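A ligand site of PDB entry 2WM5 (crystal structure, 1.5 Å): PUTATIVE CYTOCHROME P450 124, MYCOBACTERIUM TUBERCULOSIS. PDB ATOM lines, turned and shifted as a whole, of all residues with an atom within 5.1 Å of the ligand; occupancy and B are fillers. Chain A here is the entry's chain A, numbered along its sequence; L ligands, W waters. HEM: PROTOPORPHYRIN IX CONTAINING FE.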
ATOM      1  N   SER A  89      20.318 -35.484  26.735  1.00  0.00           N
ATOM      2  CA  SER A  89      20.287 -34.015  26.465  1.00  0.00           C
ATOM      3  C   SER A  89      18.856 -33.555  26.104  1.00  0.00           C
ATOM      4  O   SER A  89      18.482 -32.389  26.391  1.00  0.00           O
ATOM      5  CB  SER A  89      21.217 -33.687  25.301  1.00  0.00           C
ATOM      6  OG  SER A  89      22.554 -34.115  25.697  1.00  0.00           O
ATOM      7  N   MET A 117      22.212 -19.149  33.153  1.00  0.00           N
ATOM      8  CA  MET A 117      21.152 -20.014  32.592  1.00  0.00           C
ATOM      9  C   MET A 117      21.590 -21.498  32.540  1.00  0.00           C
ATOM     10  O   MET A 117      20.697 -22.361  32.439  1.00  0.00           O
ATOM     11  CB  MET A 117      20.831 -19.606  31.158  1.00  0.00           C
ATOM     12  CG  MET A 117      21.949 -19.733  30.171  1.00  0.00           C
ATOM     13  SD  MET A 117      21.556 -19.101  28.540  1.00  0.00           S
ATOM     14  CE  MET A 117      21.614 -17.285  28.837  1.00  0.00           C
ATOM     15  N   ILE A 118      22.870 -21.845  32.608  1.00  0.00           N
ATOM     16  CA  ILE A 118      23.306 -23.237  32.374  1.00  0.00           C
ATOM     17  C   ILE A 118      22.914 -24.148  33.541  1.00  0.00           C
ATOM     18  O   ILE A 118      22.799 -25.381  33.355  1.00  0.00           O
ATOM     19  CB  ILE A 118      24.782 -23.318  32.029  1.00  0.00           C
ATOM     20  CG1 ILE A 118      25.067 -24.544  31.141  1.00  0.00           C
ATOM     21  CG2 ILE A 118      25.722 -23.305  33.306  1.00  0.00           C
ATOM     22  CD1 ILE A 118      26.565 -24.632  30.657  1.00  0.00           C
ATOM     23  N   HIS A 125      14.946 -21.163  32.978  1.00  0.00           N
ATOM     24  CA  HIS A 125      16.032 -21.162  31.972  1.00  0.00           C
ATOM     25  C   HIS A 125      15.546 -20.469  30.691  1.00  0.00           C
ATOM     26  O   HIS A 125      16.261 -19.588  30.145  1.00  0.00           O
ATOM     27  CB  HIS A 125      16.425 -22.650  31.676  1.00  0.00           C
ATOM     28  CG  HIS A 125      17.170 -22.818  30.398  1.00  0.00           C
ATOM     29  ND1 HIS A 125      16.559 -23.162  29.200  1.00  0.00           N
ATOM     30  CD2 HIS A 125      18.490 -22.616  30.129  1.00  0.00           C
ATOM     31  CE1 HIS A 125      17.493 -23.161  28.237  1.00  0.00           C
ATOM     32  NE2 HIS A 125      18.655 -22.826  28.779  1.00  0.00           N
ATOM     33  N   ARG A 129      17.264 -17.301  28.849  1.00  0.00           N
ATOM     34  CA  ARG A 129      17.890 -17.510  27.545  1.00  0.00           C
ATOM     35  C   ARG A 129      17.167 -16.700  26.464  1.00  0.00           C
ATOM     36  O   ARG A 129      17.849 -16.108  25.565  1.00  0.00           O
ATOM     37  CB  ARG A 129      17.900 -19.023  27.173  1.00  0.00           C
ATOM     38  CG  ARG A 129      18.559 -19.243  25.816  1.00  0.00           C
ATOM     39  CD  ARG A 129      18.790 -20.726  25.617  1.00  0.00           C
ATOM     40  NE  ARG A 129      19.252 -20.930  24.235  1.00  0.00           N
ATOM     41  CZ  ARG A 129      20.248 -21.721  23.878  1.00  0.00           C
ATOM     42  NH1 ARG A 129      20.974 -22.347  24.805  1.00  0.00           N
ATOM     43  NH2 ARG A 129      20.614 -21.794  22.568  1.00  0.00           N
ATOM     44  N   ILE A 183      35.170 -11.106  24.216  1.00  0.00           N
ATOM     45  CA  ILE A 183      34.075 -10.891  25.160  1.00  0.00           C
ATOM     46  C   ILE A 183      34.148  -9.414  25.721  1.00  0.00           C
ATOM     47  O   ILE A 183      33.085  -8.777  25.889  1.00  0.00           O
ATOM     48  CB  ILE A 183      34.134 -11.901  26.316  1.00  0.00           C
ATOM     49  CG1 ILE A 183      33.630 -13.289  25.834  1.00  0.00           C
ATOM     50  CG2 ILE A 183      33.342 -11.424  27.574  1.00  0.00           C
ATOM     51  CD1 ILE A 183      34.150 -14.451  26.733  1.00  0.00           C
ATOM     52  N   MET A 186      32.742  -7.194  23.048  1.00  0.00           N
ATOM     53  CA  MET A 186      31.303  -7.420  22.880  1.00  0.00           C
ATOM     54  C   MET A 186      30.513  -6.680  23.986  1.00  0.00           C
ATOM     55  O   MET A 186      29.449  -6.067  23.736  1.00  0.00           O
ATOM     56  CB  MET A 186      31.058  -8.945  23.059  1.00  0.00           C
ATOM     57  CG  MET A 186      29.570  -9.312  23.035  1.00  0.00           C
ATOM     58  SD  MET A 186      29.417 -11.099  22.795  1.00  0.00           S
ATOM     59  CE  MET A 186      29.948 -11.632  24.403  1.00  0.00           C
ATOM     60  N   PHE A 267      25.431 -13.676  33.930  1.00  0.00           N
ATOM     61  CA  PHE A 267      25.611 -14.085  32.544  1.00  0.00           C
ATOM     62  C   PHE A 267      27.079 -13.756  32.147  1.00  0.00           C
ATOM     63  O   PHE A 267      27.755 -14.565  31.462  1.00  0.00           O
ATOM     64  CB  PHE A 267      24.567 -13.405  31.613  1.00  0.00           C
ATOM     65  CG  PHE A 267      24.780 -13.734  30.189  1.00  0.00           C
ATOM     66  CD1 PHE A 267      24.657 -15.043  29.733  1.00  0.00           C
ATOM     67  CD2 PHE A 267      25.116 -12.736  29.259  1.00  0.00           C
ATOM     68  CE1 PHE A 267      24.884 -15.356  28.423  1.00  0.00           C
ATOM     69  CE2 PHE A 267      25.375 -13.073  27.940  1.00  0.00           C
ATOM     70  CZ  PHE A 267      25.268 -14.350  27.509  1.00  0.00           C
ATOM     71  N   LEU A 270      29.386 -16.312  33.598  1.00  0.00           N
ATOM     72  CA  LEU A 270      29.302 -17.529  32.764  1.00  0.00           C
ATOM     73  C   LEU A 270      30.151 -17.353  31.518  1.00  0.00           C
ATOM     74  O   LEU A 270      30.946 -18.284  31.166  1.00  0.00           O
ATOM     75  CB  LEU A 270      27.820 -17.864  32.415  1.00  0.00           C
ATOM     76  CG  LEU A 270      27.685 -19.049  31.420  1.00  0.00           C
ATOM     77  CD1 LEU A 270      28.121 -20.375  32.062  1.00  0.00           C
ATOM     78  CD2 LEU A 270      26.195 -19.149  31.025  1.00  0.00           C
ATOM     79  N   LEU A 271      30.003 -16.197  30.844  1.00  0.00           N
ATOM     80  CA  LEU A 271      30.748 -16.058  29.547  1.00  0.00           C
ATOM     81  C   LEU A 271      32.271 -16.133  29.747  1.00  0.00           C
ATOM     82  O   LEU A 271      32.961 -16.766  28.891  1.00  0.00           O
ATOM     83  CB  LEU A 271      30.424 -14.721  28.888  1.00  0.00           C
ATOM     84  CG  LEU A 271      29.028 -14.550  28.360  1.00  0.00           C
ATOM     85  CD1 LEU A 271      28.963 -13.218  27.576  1.00  0.00           C
ATOM     86  CD2 LEU A 271      28.652 -15.747  27.484  1.00  0.00           C
ATOM     87  N   ALA A 274      32.722 -20.163  30.342  1.00  0.00           N
ATOM     88  CA  ALA A 274      32.164 -21.081  29.343  1.00  0.00           C
ATOM     89  C   ALA A 274      32.338 -20.640  27.887  1.00  0.00           C
ATOM     90  O   ALA A 274      32.324 -21.492  26.979  1.00  0.00           O
ATOM     91  CB  ALA A 274      30.650 -21.362  29.666  1.00  0.00           C
ATOM     92  N   GLY A 275      32.433 -19.324  27.661  1.00  0.00           N
ATOM     93  CA  GLY A 275      32.653 -18.772  26.341  1.00  0.00           C
ATOM     94  C   GLY A 275      34.082 -18.397  26.079  1.00  0.00           C
ATOM     95  O   GLY A 275      34.407 -17.674  25.098  1.00  0.00           O
ATOM     96  N   THR A 278      36.762 -22.669  26.576  1.00  0.00           N
ATOM     97  CA  THR A 278      36.344 -23.651  25.575  1.00  0.00           C
ATOM     98  C   THR A 278      36.935 -23.240  24.192  1.00  0.00           C
ATOM     99  O   THR A 278      37.594 -24.065  23.541  1.00  0.00           O
ATOM    100  CB  THR A 278      34.821 -23.621  25.448  1.00  0.00           C
ATOM    101  OG1 THR A 278      34.381 -22.228  25.322  1.00  0.00           O
ATOM    102  CG2 THR A 278      34.166 -24.292  26.707  1.00  0.00           C
ATOM    103  N   THR A 279      36.651 -22.031  23.741  1.00  0.00           N
ATOM    104  CA  THR A 279      37.221 -21.627  22.415  1.00  0.00           C
ATOM    105  C   THR A 279      38.752 -21.659  22.429  1.00  0.00           C
ATOM    106  O   THR A 279      39.368 -22.122  21.412  1.00  0.00           O
ATOM    107  CB  THR A 279      36.774 -20.181  22.086  1.00  0.00           C
ATOM    108  OG1 THR A 279      35.333 -20.195  22.090  1.00  0.00           O
ATOM    109  CG2 THR A 279      37.309 -19.721  20.727  1.00  0.00           C
ATOM    110  N   ALA A 282      39.654 -25.276  21.842  1.00  0.00           N
ATOM    111  CA  ALA A 282      39.375 -25.688  20.447  1.00  0.00           C
ATOM    112  C   ALA A 282      40.547 -25.208  19.532  1.00  0.00           C
ATOM    113  O   ALA A 282      41.017 -25.984  18.670  1.00  0.00           O
ATOM    114  CB  ALA A 282      38.039 -25.099  19.927  1.00  0.00           C
ATOM    115  N   VAL A 316      36.146 -29.029  16.388  1.00  0.00           N
ATOM    116  CA  VAL A 316      35.375 -29.140  17.641  1.00  0.00           C
ATOM    117  C   VAL A 316      35.122 -30.626  18.006  1.00  0.00           C
ATOM    118  O   VAL A 316      35.239 -31.036  19.188  1.00  0.00           O
ATOM    119  CB  VAL A 316      34.057 -28.311  17.575  1.00  0.00           C
ATOM    120  CG1 VAL A 316      33.221 -28.466  18.854  1.00  0.00           C
ATOM    121  CG2 VAL A 316      34.397 -26.798  17.377  1.00  0.00           C
ATOM    122  N   PRO A 321      36.221 -29.713  23.562  1.00  0.00           N
ATOM    123  CA  PRO A 321      36.812 -28.877  24.645  1.00  0.00           C
ATOM    124  C   PRO A 321      36.091 -29.106  25.986  1.00  0.00           C
ATOM    125  O   PRO A 321      36.730 -29.004  27.056  1.00  0.00           O
ATOM    126  CB  PRO A 321      36.580 -27.403  24.197  1.00  0.00           C
ATOM    127  CG  PRO A 321      36.558 -27.611  22.584  1.00  0.00           C
ATOM    128  CD  PRO A 321      35.803 -28.921  22.380  1.00  0.00           C
ATOM    129  N   VAL A 322      34.785 -29.365  25.920  1.00  0.00           N
ATOM    130  CA  VAL A 322      33.995 -29.662  27.155  1.00  0.00           C
ATOM    131  C   VAL A 322      33.957 -31.185  27.113  1.00  0.00           C
ATOM    132  O   VAL A 322      33.289 -31.828  26.296  1.00  0.00           O
ATOM    133  CB  VAL A 322      32.554 -29.080  27.084  1.00  0.00           C
ATOM    134  CG1 VAL A 322      31.769 -29.508  28.323  1.00  0.00           C
ATOM    135  CG2 VAL A 322      32.645 -27.552  27.052  1.00  0.00           C
ATOM    136  N   MET A 325      29.168 -33.013  30.479  1.00  0.00           N
ATOM    137  CA  MET A 325      28.335 -32.186  31.392  1.00  0.00           C
ATOM    138  C   MET A 325      27.554 -33.171  32.265  1.00  0.00           C
ATOM    139  O   MET A 325      27.239 -34.300  31.791  1.00  0.00           O
ATOM    140  CB  MET A 325      27.359 -31.260  30.642  1.00  0.00           C
ATOM    141  CG  MET A 325      28.162 -30.113  30.015  1.00  0.00           C
ATOM    142  SD  MET A 325      28.182 -28.740  31.244  1.00  0.00           S
ATOM    143  CE  MET A 325      29.152 -27.541  30.291  1.00  0.00           C
ATOM    144  N   ARG A 327      24.114 -34.153  34.758  1.00  0.00           N
ATOM    145  CA  ARG A 327      22.697 -33.935  35.044  1.00  0.00           C
ATOM    146  C   ARG A 327      22.338 -34.672  36.292  1.00  0.00           C
ATOM    147  O   ARG A 327      23.117 -35.497  36.812  1.00  0.00           O
ATOM    148  CB  ARG A 327      21.867 -34.556  33.876  1.00  0.00           C
ATOM    149  CG  ARG A 327      22.070 -33.870  32.488  1.00  0.00           C
ATOM    150  CD  ARG A 327      21.564 -32.413  32.463  1.00  0.00           C
ATOM    151  NE  ARG A 327      21.616 -31.809  31.117  1.00  0.00           N
ATOM    152  CZ  ARG A 327      22.560 -30.963  30.667  1.00  0.00           C
ATOM    153  NH1 ARG A 327      23.652 -30.763  31.367  1.00  0.00           N
ATOM    154  NH2 ARG A 327      22.409 -30.365  29.474  1.00  0.00           N
ATOM    155  N   TYR A 350      30.781 -36.162  26.211  1.00  0.00           N
ATOM    156  CA  TYR A 350      30.861 -35.725  24.841  1.00  0.00           C
ATOM    157  C   TYR A 350      32.166 -36.226  24.194  1.00  0.00           C
ATOM    158  O   TYR A 350      32.185 -36.534  23.002  1.00  0.00           O
ATOM    159  CB  TYR A 350      30.927 -34.161  24.802  1.00  0.00           C
ATOM    160  CG  TYR A 350      29.729 -33.542  25.515  1.00  0.00           C
ATOM    161  CD1 TYR A 350      28.410 -33.996  25.259  1.00  0.00           C
ATOM    162  CD2 TYR A 350      29.929 -32.494  26.454  1.00  0.00           C
ATOM    163  CE1 TYR A 350      27.308 -33.386  25.909  1.00  0.00           C
ATOM    164  CE2 TYR A 350      28.848 -31.869  27.083  1.00  0.00           C
ATOM    165  CZ  TYR A 350      27.556 -32.317  26.820  1.00  0.00           C
ATOM    166  OH  TYR A 350      26.528 -31.661  27.448  1.00  0.00           O
ATOM    167  N   GLY A 377      30.138 -31.759  20.435  1.00  0.00           N
ATOM    168  CA  GLY A 377      31.063 -30.916  21.115  1.00  0.00           C
ATOM    169  C   GLY A 377      30.401 -29.681  21.705  1.00  0.00           C
ATOM    170  O   GLY A 377      30.883 -29.189  22.764  1.00  0.00           O
ATOM    171  N   PHE A 378      29.242 -29.241  21.178  1.00  0.00           N
ATOM    172  CA  PHE A 378      28.455 -28.154  21.802  1.00  0.00           C
ATOM    173  C   PHE A 378      27.282 -28.716  22.576  1.00  0.00           C
ATOM    174  O   PHE A 378      26.269 -28.055  22.834  1.00  0.00           O
ATOM    175  CB  PHE A 378      27.907 -27.227  20.688  1.00  0.00           C
ATOM    176  CG  PHE A 378      28.996 -26.468  19.946  1.00  0.00           C
ATOM    177  CD1 PHE A 378      29.777 -25.529  20.610  1.00  0.00           C
ATOM    178  CD2 PHE A 378      29.211 -26.698  18.575  1.00  0.00           C
ATOM    179  CE1 PHE A 378      30.753 -24.744  19.937  1.00  0.00           C
ATOM    180  CE2 PHE A 378      30.113 -25.944  17.857  1.00  0.00           C
ATOM    181  CZ  PHE A 378      30.972 -25.013  18.549  1.00  0.00           C
ATOM    182  N   GLY A 379      27.426 -30.007  22.949  1.00  0.00           N
ATOM    183  CA  GLY A 379      26.370 -30.769  23.673  1.00  0.00           C
ATOM    184  C   GLY A 379      25.453 -31.535  22.757  1.00  0.00           C
ATOM    185  O   GLY A 379      25.624 -31.555  21.488  1.00  0.00           O
ATOM    186  N   GLY A 380      24.498 -32.291  23.365  1.00  0.00           N
ATOM    187  CA  GLY A 380      23.637 -33.123  22.549  1.00  0.00           C
ATOM    188  C   GLY A 380      22.487 -32.478  21.853  1.00  0.00           C
ATOM    189  O   GLY A 380      21.623 -33.214  21.281  1.00  0.00           O
ATOM    190  N   GLY A 381      22.380 -31.161  21.977  1.00  0.00           N
ATOM    191  CA  GLY A 381      21.224 -30.423  21.409  1.00  0.00           C
ATOM    192  C   GLY A 381      20.147 -30.260  22.436  1.00  0.00           C
ATOM    193  O   GLY A 381      20.250 -30.814  23.599  1.00  0.00           O
ATOM    194  N   ALA A 383      17.551 -28.018  24.944  1.00  0.00           N
ATOM    195  CA  ALA A 383      17.276 -26.755  25.601  1.00  0.00           C
ATOM    196  C   ALA A 383      18.551 -25.925  25.895  1.00  0.00           C
ATOM    197  O   ALA A 383      18.481 -24.675  25.913  1.00  0.00           O
ATOM    198  CB  ALA A 383      16.506 -27.044  26.940  1.00  0.00           C
ATOM    199  N   HIS A 384      19.647 -26.600  26.268  1.00  0.00           N
ATOM    200  CA  HIS A 384      20.866 -25.909  26.658  1.00  0.00           C
ATOM    201  C   HIS A 384      21.891 -25.862  25.545  1.00  0.00           C
ATOM    202  O   HIS A 384      23.060 -25.488  25.820  1.00  0.00           O
ATOM    203  CB  HIS A 384      21.444 -26.573  27.913  1.00  0.00           C
ATOM    204  CG  HIS A 384      20.602 -26.379  29.131  1.00  0.00           C
ATOM    205  ND1 HIS A 384      20.667 -25.225  29.933  1.00  0.00           N
ATOM    206  CD2 HIS A 384      19.660 -27.204  29.735  1.00  0.00           C
ATOM    207  CE1 HIS A 384      19.837 -25.374  30.975  1.00  0.00           C
ATOM    208  NE2 HIS A 384      19.214 -26.563  30.853  1.00  0.00           N
ATOM    209  N   PHE A 385      21.524 -26.157  24.293  1.00  0.00           N
ATOM    210  CA  PHE A 385      22.535 -26.197  23.227  1.00  0.00           C
ATOM    211  C   PHE A 385      23.374 -24.890  23.246  1.00  0.00           C
ATOM    212  O   PHE A 385      22.786 -23.779  23.292  1.00  0.00           O
ATOM    213  CB  PHE A 385      21.867 -26.345  21.835  1.00  0.00           C
ATOM    214  CG  PHE A 385      22.908 -26.399  20.760  1.00  0.00           C
ATOM    215  CD1 PHE A 385      23.596 -27.589  20.480  1.00  0.00           C
ATOM    216  CD2 PHE A 385      23.241 -25.203  20.069  1.00  0.00           C
ATOM    217  CE1 PHE A 385      24.689 -27.622  19.552  1.00  0.00           C
ATOM    218  CE2 PHE A 385      24.286 -25.233  19.103  1.00  0.00           C
ATOM    219  CZ  PHE A 385      25.053 -26.433  18.910  1.00  0.00           C
ATOM    220  N   CYS A 386      24.700 -25.026  23.178  1.00  0.00           N
ATOM    221  CA  CYS A 386      25.590 -23.841  23.342  1.00  0.00           C
ATOM    222  C   CYS A 386      25.068 -22.581  22.665  1.00  0.00           C
ATOM    223  O   CYS A 386      24.902 -22.522  21.397  1.00  0.00           O
ATOM    224  CB  CYS A 386      26.921 -24.223  22.660  1.00  0.00           C
ATOM    225  SG  CYS A 386      28.072 -22.815  22.797  1.00  0.00           S
ATOM    226  N   LEU A 387      24.777 -21.556  23.493  1.00  0.00           N
ATOM    227  CA  LEU A 387      24.220 -20.322  22.966  1.00  0.00           C
ATOM    228  C   LEU A 387      25.279 -19.593  22.122  1.00  0.00           C
ATOM    229  O   LEU A 387      24.886 -18.881  21.161  1.00  0.00           O
ATOM    230  CB  LEU A 387      23.817 -19.400  24.119  1.00  0.00           C
ATOM    231  CG  LEU A 387      23.151 -18.071  23.697  1.00  0.00           C
ATOM    232  CD1 LEU A 387      21.855 -18.342  22.885  1.00  0.00           C
ATOM    233  CD2 LEU A 387      22.659 -17.377  24.982  1.00  0.00           C
ATOM    234  N   GLY A 388      26.561 -19.828  22.359  1.00  0.00           N
ATOM    235  CA  GLY A 388      27.632 -19.175  21.636  1.00  0.00           C
ATOM    236  C   GLY A 388      28.151 -19.952  20.467  1.00  0.00           C
ATOM    237  O   GLY A 388      29.224 -19.579  19.976  1.00  0.00           O
ATOM    238  N   ALA A 389      27.463 -21.041  20.026  1.00  0.00           N
ATOM    239  CA  ALA A 389      28.120 -21.950  19.095  1.00  0.00           C
ATOM    240  C   ALA A 389      28.527 -21.192  17.819  1.00  0.00           C
ATOM    241  O   ALA A 389      29.633 -21.452  17.275  1.00  0.00           O
ATOM    242  CB  ALA A 389      27.255 -23.170  18.754  1.00  0.00           C
ATOM    243  N   LEU A 391      29.232 -18.009  17.418  1.00  0.00           N
ATOM    244  CA  LEU A 391      30.389 -17.130  17.724  1.00  0.00           C
ATOM    245  C   LEU A 391      31.661 -18.003  17.861  1.00  0.00           C
ATOM    246  O   LEU A 391      32.724 -17.660  17.336  1.00  0.00           O
ATOM    247  CB  LEU A 391      30.113 -16.347  19.038  1.00  0.00           C
ATOM    248  CG  LEU A 391      31.371 -15.565  19.556  1.00  0.00           C
ATOM    249  CD1 LEU A 391      31.871 -14.650  18.484  1.00  0.00           C
ATOM    250  CD2 LEU A 391      30.931 -14.750  20.844  1.00  0.00           C
ATOM    251  N   ALA A 392      31.543 -19.149  18.552  1.00  0.00           N
ATOM    252  CA  ALA A 392      32.730 -20.026  18.677  1.00  0.00           C
ATOM    253  C   ALA A 392      33.235 -20.465  17.280  1.00  0.00           C
ATOM    254  O   ALA A 392      34.466 -20.474  17.019  1.00  0.00           O
ATOM    255  CB  ALA A 392      32.389 -21.314  19.510  1.00  0.00           C
ATOM    256  N   GLU A 395      35.038 -17.577  15.748  1.00  0.00           N
ATOM    257  CA  GLU A 395      36.329 -17.369  16.421  1.00  0.00           C
ATOM    258  C   GLU A 395      37.390 -18.392  15.911  1.00  0.00           C
ATOM    259  O   GLU A 395      38.544 -18.028  15.647  1.00  0.00           O
ATOM    260  CB  GLU A 395      36.228 -17.453  17.941  1.00  0.00           C
ATOM    261  CG  GLU A 395      35.350 -16.341  18.554  1.00  0.00           C
ATOM    262  CD  GLU A 395      35.124 -16.506  20.027  1.00  0.00           C
ATOM    263  OE1 GLU A 395      34.931 -17.684  20.510  1.00  0.00           O
ATOM    264  OE2 GLU A 395      34.836 -15.490  20.671  1.00  0.00           O
ATOM    265  N   ILE A 396      36.986 -19.664  15.814  1.00  0.00           N
ATOM    266  CA  ILE A 396      37.885 -20.711  15.350  1.00  0.00           C
ATOM    267  C   ILE A 396      38.287 -20.391  13.894  1.00  0.00           C
ATOM    268  O   ILE A 396      39.468 -20.353  13.545  1.00  0.00           O
ATOM    269  CB  ILE A 396      37.310 -22.123  15.527  1.00  0.00           C
ATOM    270  CG1 ILE A 396      37.104 -22.360  17.046  1.00  0.00           C
ATOM    271  CG2 ILE A 396      38.220 -23.177  14.884  1.00  0.00           C
ATOM    272  CD1 ILE A 396      36.109 -23.558  17.271  1.00  0.00           C
HETATM  273  CHA HEM L   1      26.504 -23.985  26.859  1.00  0.00           C
HETATM  274  CHB HEM L   1      30.310 -26.055  24.547  1.00  0.00           C
HETATM  275  CHC HEM L   1      31.816 -21.592  23.182  1.00  0.00           C
HETATM  276  CHD HEM L   1      28.127 -19.482  25.543  1.00  0.00           C
HETATM  277  C1A HEM L   1      27.402 -24.918  26.368  1.00  0.00           C
HETATM  278  C2A HEM L   1      27.317 -26.352  26.545  1.00  0.00           C
HETATM  279  C3A HEM L   1      28.376 -26.930  25.924  1.00  0.00           C
HETATM  280  C4A HEM L   1      29.166 -25.867  25.299  1.00  0.00           C
HETATM  281  CMA HEM L   1      28.782 -28.442  25.873  1.00  0.00           C
HETATM  282  CAA HEM L   1      26.264 -27.078  27.358  1.00  0.00           C
HETATM  283  CBA HEM L   1      25.297 -27.731  26.295  1.00  0.00           C
HETATM  284  CGA HEM L   1      24.235 -28.650  26.909  1.00  0.00           C
HETATM  285  O1A HEM L   1      24.202 -28.755  28.152  1.00  0.00           O
HETATM  286  O2A HEM L   1      23.437 -29.272  26.174  1.00  0.00           O
HETATM  287  C1B HEM L   1      31.072 -25.014  24.018  1.00  0.00           C
HETATM  288  C2B HEM L   1      32.247 -25.203  23.213  1.00  0.00           C
HETATM  289  C3B HEM L   1      32.661 -23.919  22.823  1.00  0.00           C
HETATM  290  C4B HEM L   1      31.784 -22.946  23.390  1.00  0.00           C
HETATM  291  CMB HEM L   1      32.899 -26.590  22.904  1.00  0.00           C
HETATM  292  CAB HEM L   1      33.873 -23.528  21.984  1.00  0.00           C
HETATM  293  CBB HEM L   1      34.412 -24.272  20.993  1.00  0.00           C
HETATM  294  C1C HEM L   1      30.964 -20.661  23.676  1.00  0.00           C
HETATM  295  C2C HEM L   1      31.053 -19.213  23.445  1.00  0.00           C
HETATM  296  C3C HEM L   1      29.997 -18.675  24.073  1.00  0.00           C
HETATM  297  C4C HEM L   1      29.293 -19.718  24.806  1.00  0.00           C
HETATM  298  CMC HEM L   1      32.107 -18.529  22.500  1.00  0.00           C
HETATM  299  CAC HEM L   1      29.582 -17.210  24.192  1.00  0.00           C
HETATM  300  CBC HEM L   1      30.583 -16.309  24.174  1.00  0.00           C
HETATM  301  C1D HEM L   1      27.376 -20.545  26.119  1.00  0.00           C
HETATM  302  C2D HEM L   1      26.210 -20.316  26.959  1.00  0.00           C
HETATM  303  C3D HEM L   1      25.727 -21.662  27.324  1.00  0.00           C
HETATM  304  C4D HEM L   1      26.603 -22.611  26.691  1.00  0.00           C
HETATM  305  CMD HEM L   1      25.626 -18.964  27.381  1.00  0.00           C
HETATM  306  CAD HEM L   1      24.524 -21.993  28.213  1.00  0.00           C
HETATM  307  CBD HEM L   1      23.360 -22.241  27.246  1.00  0.00           C
HETATM  308  CGD HEM L   1      22.140 -22.722  28.043  1.00  0.00           C
HETATM  309  O1D HEM L   1      22.284 -23.196  29.195  1.00  0.00           O
HETATM  310  O2D HEM L   1      20.951 -22.627  27.557  1.00  0.00           O
HETATM  311  NA  HEM L   1      28.542 -24.625  25.577  1.00  0.00           N
HETATM  312  NB  HEM L   1      30.804 -23.641  24.087  1.00  0.00           N
HETATM  313  NC  HEM L   1      29.848 -20.938  24.459  1.00  0.00           N
HETATM  314  ND  HEM L   1      27.647 -21.925  26.006  1.00  0.00           N
HETATM  315 FE   HEM L   1      29.107 -22.784  24.878  1.00  0.00          FE
HETATM  316  O   HOH W   1      24.178 -31.868  26.209  1.00  0.00           O
HETATM  317  O   HOH W   2      25.065 -28.362  30.602  1.00  0.00           O
HETATM  318  O   HOH W   3      20.644 -29.402  25.971  1.00  0.00           O
HETATM  319  O   HOH W   4      23.682 -29.184  23.408  1.00  0.00           O
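SG of Cys 386 binds FE of the ligand.
A ring nitrogen (NE2) of His 125 lies within hydrogen-bond range of an oxygen (O2D) of the ligand, at 2.6 Å.
ND1 of His 384 is in hydrogen-bond range of O1D of the ligand (2.7 Å).
O1A of the ligand lies within salt-bridge range of NH2 of Arg 327.
The guanidinium group of Arg 129 is in salt-bridge range of an oxygen (O2D) of the ligand, 2.8 Å away.
N of Gly 388 sits close to SG of Cys 386.
N of Cys 386 is in hydrogen-bond range of O of Phe 378, at 3.4 Å.
The backbone NH of Ala 389 lies close to the side-chain sulfur of Cys 386 (3.3 Å).
A ring nitrogen (NE2) of His 125 sits at hydrogen-bond distance from a ring nitrogen (ND1) of His 384, at 3.3 Å.
The backbone carbonyl oxygen of Ala 383 lies close to a ring nitrogen (NE2) of His 125 (3.4 Å).
NH1 of Arg 129 is in hydrogen-bond range of O of Phe 385, at 2.8 Å.
The backbone carbonyl oxygen (O) of Ala 274 lies within hydrogen-bond range of the side-chain hydroxyl (OG1) of Thr 278.
The side-chain hydroxyl (OG1) of Thr 279 lies within hydrogen-bond range of the side-chain carboxylate (OE1) of Glu 395 (3.0 Å).
The side-chain sulfur (SD) of Met 117 lies close to an oxygen (O2D) of the ligand, at 3.7 Å.
CA of Ile 118 touches O1D of the ligand, 3.3 Å away.
Phe 267 touches the ligand.
Leu 270 touches the ligand.
Leu 271 touches the ligand.
Ala 274 touches the ligand (O to NC, 3.6 Å).
CA of Gly 275 touches C2C of the ligand, at 3.3 Å.
Thr 278 touches the ligand.
Thr 279 touches the ligand.
Ala 282 touches the ligand.
Pro 321 touches the ligand.
CG2 of Val 322 touches CHB of the ligand, at 3.7 Å.
CE2 of Tyr 350 touches CMA of the ligand, 3.6 Å away.
Gly 377 touches the ligand.
Phe 378 touches the ligand.
Gly 379 touches the ligand.
Ala 383 touches the ligand.
Leu 387 touches the ligand (CB to CMD, 3.8 Å).
Gly 388 touches the ligand.
Leu 391 touches the ligand (CD2 to CBC, 3.7 Å).
CB of Ala 392 touches CAB of the ligand, 3.6 Å away.
Glu 395 touches the ligand.
Hydrophobic or aromatic side chains that line the ligand: Met 117, Ile 118, His 125, Phe 267, Leu 270, Leu 271, Ala 282, Pro 321, Val 322, Tyr 350, Phe 378, His 384, Leu 387, Leu 391 and Ala 392.
The nearest printed residue that does not touch the ligand is Phe 385 (4.1 Å).
Water W2 lies within hydrogen-bond range of an oxygen (O1A) of the ligand (2.6 Å), the guanidinium group of Arg 327 (2.9 Å) and the side-chain sulfur of Met 325 (3.2 Å).
Water W1 lies within hydrogen-bond range of the side-chain hydroxyl (OH) of Tyr 350 (2.7 Å), an oxygen (O2A) of the ligand (2.7 Å), the side-chain hydroxyl (OG) of Ser 89 (2.8 Å) and the backbone NH (N) of Gly 380 (2.9 Å).
Water W4 lies within hydrogen-bond range of the backbone NH of Gly 381, an oxygen (O2A) of the ligand, the backbone carbonyl oxygen of Phe 378 and the backbone NH of Gly 380.
Water W3 lies within hydrogen-bond range of O of Gly 381, O2A of the ligand and N of His 384.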
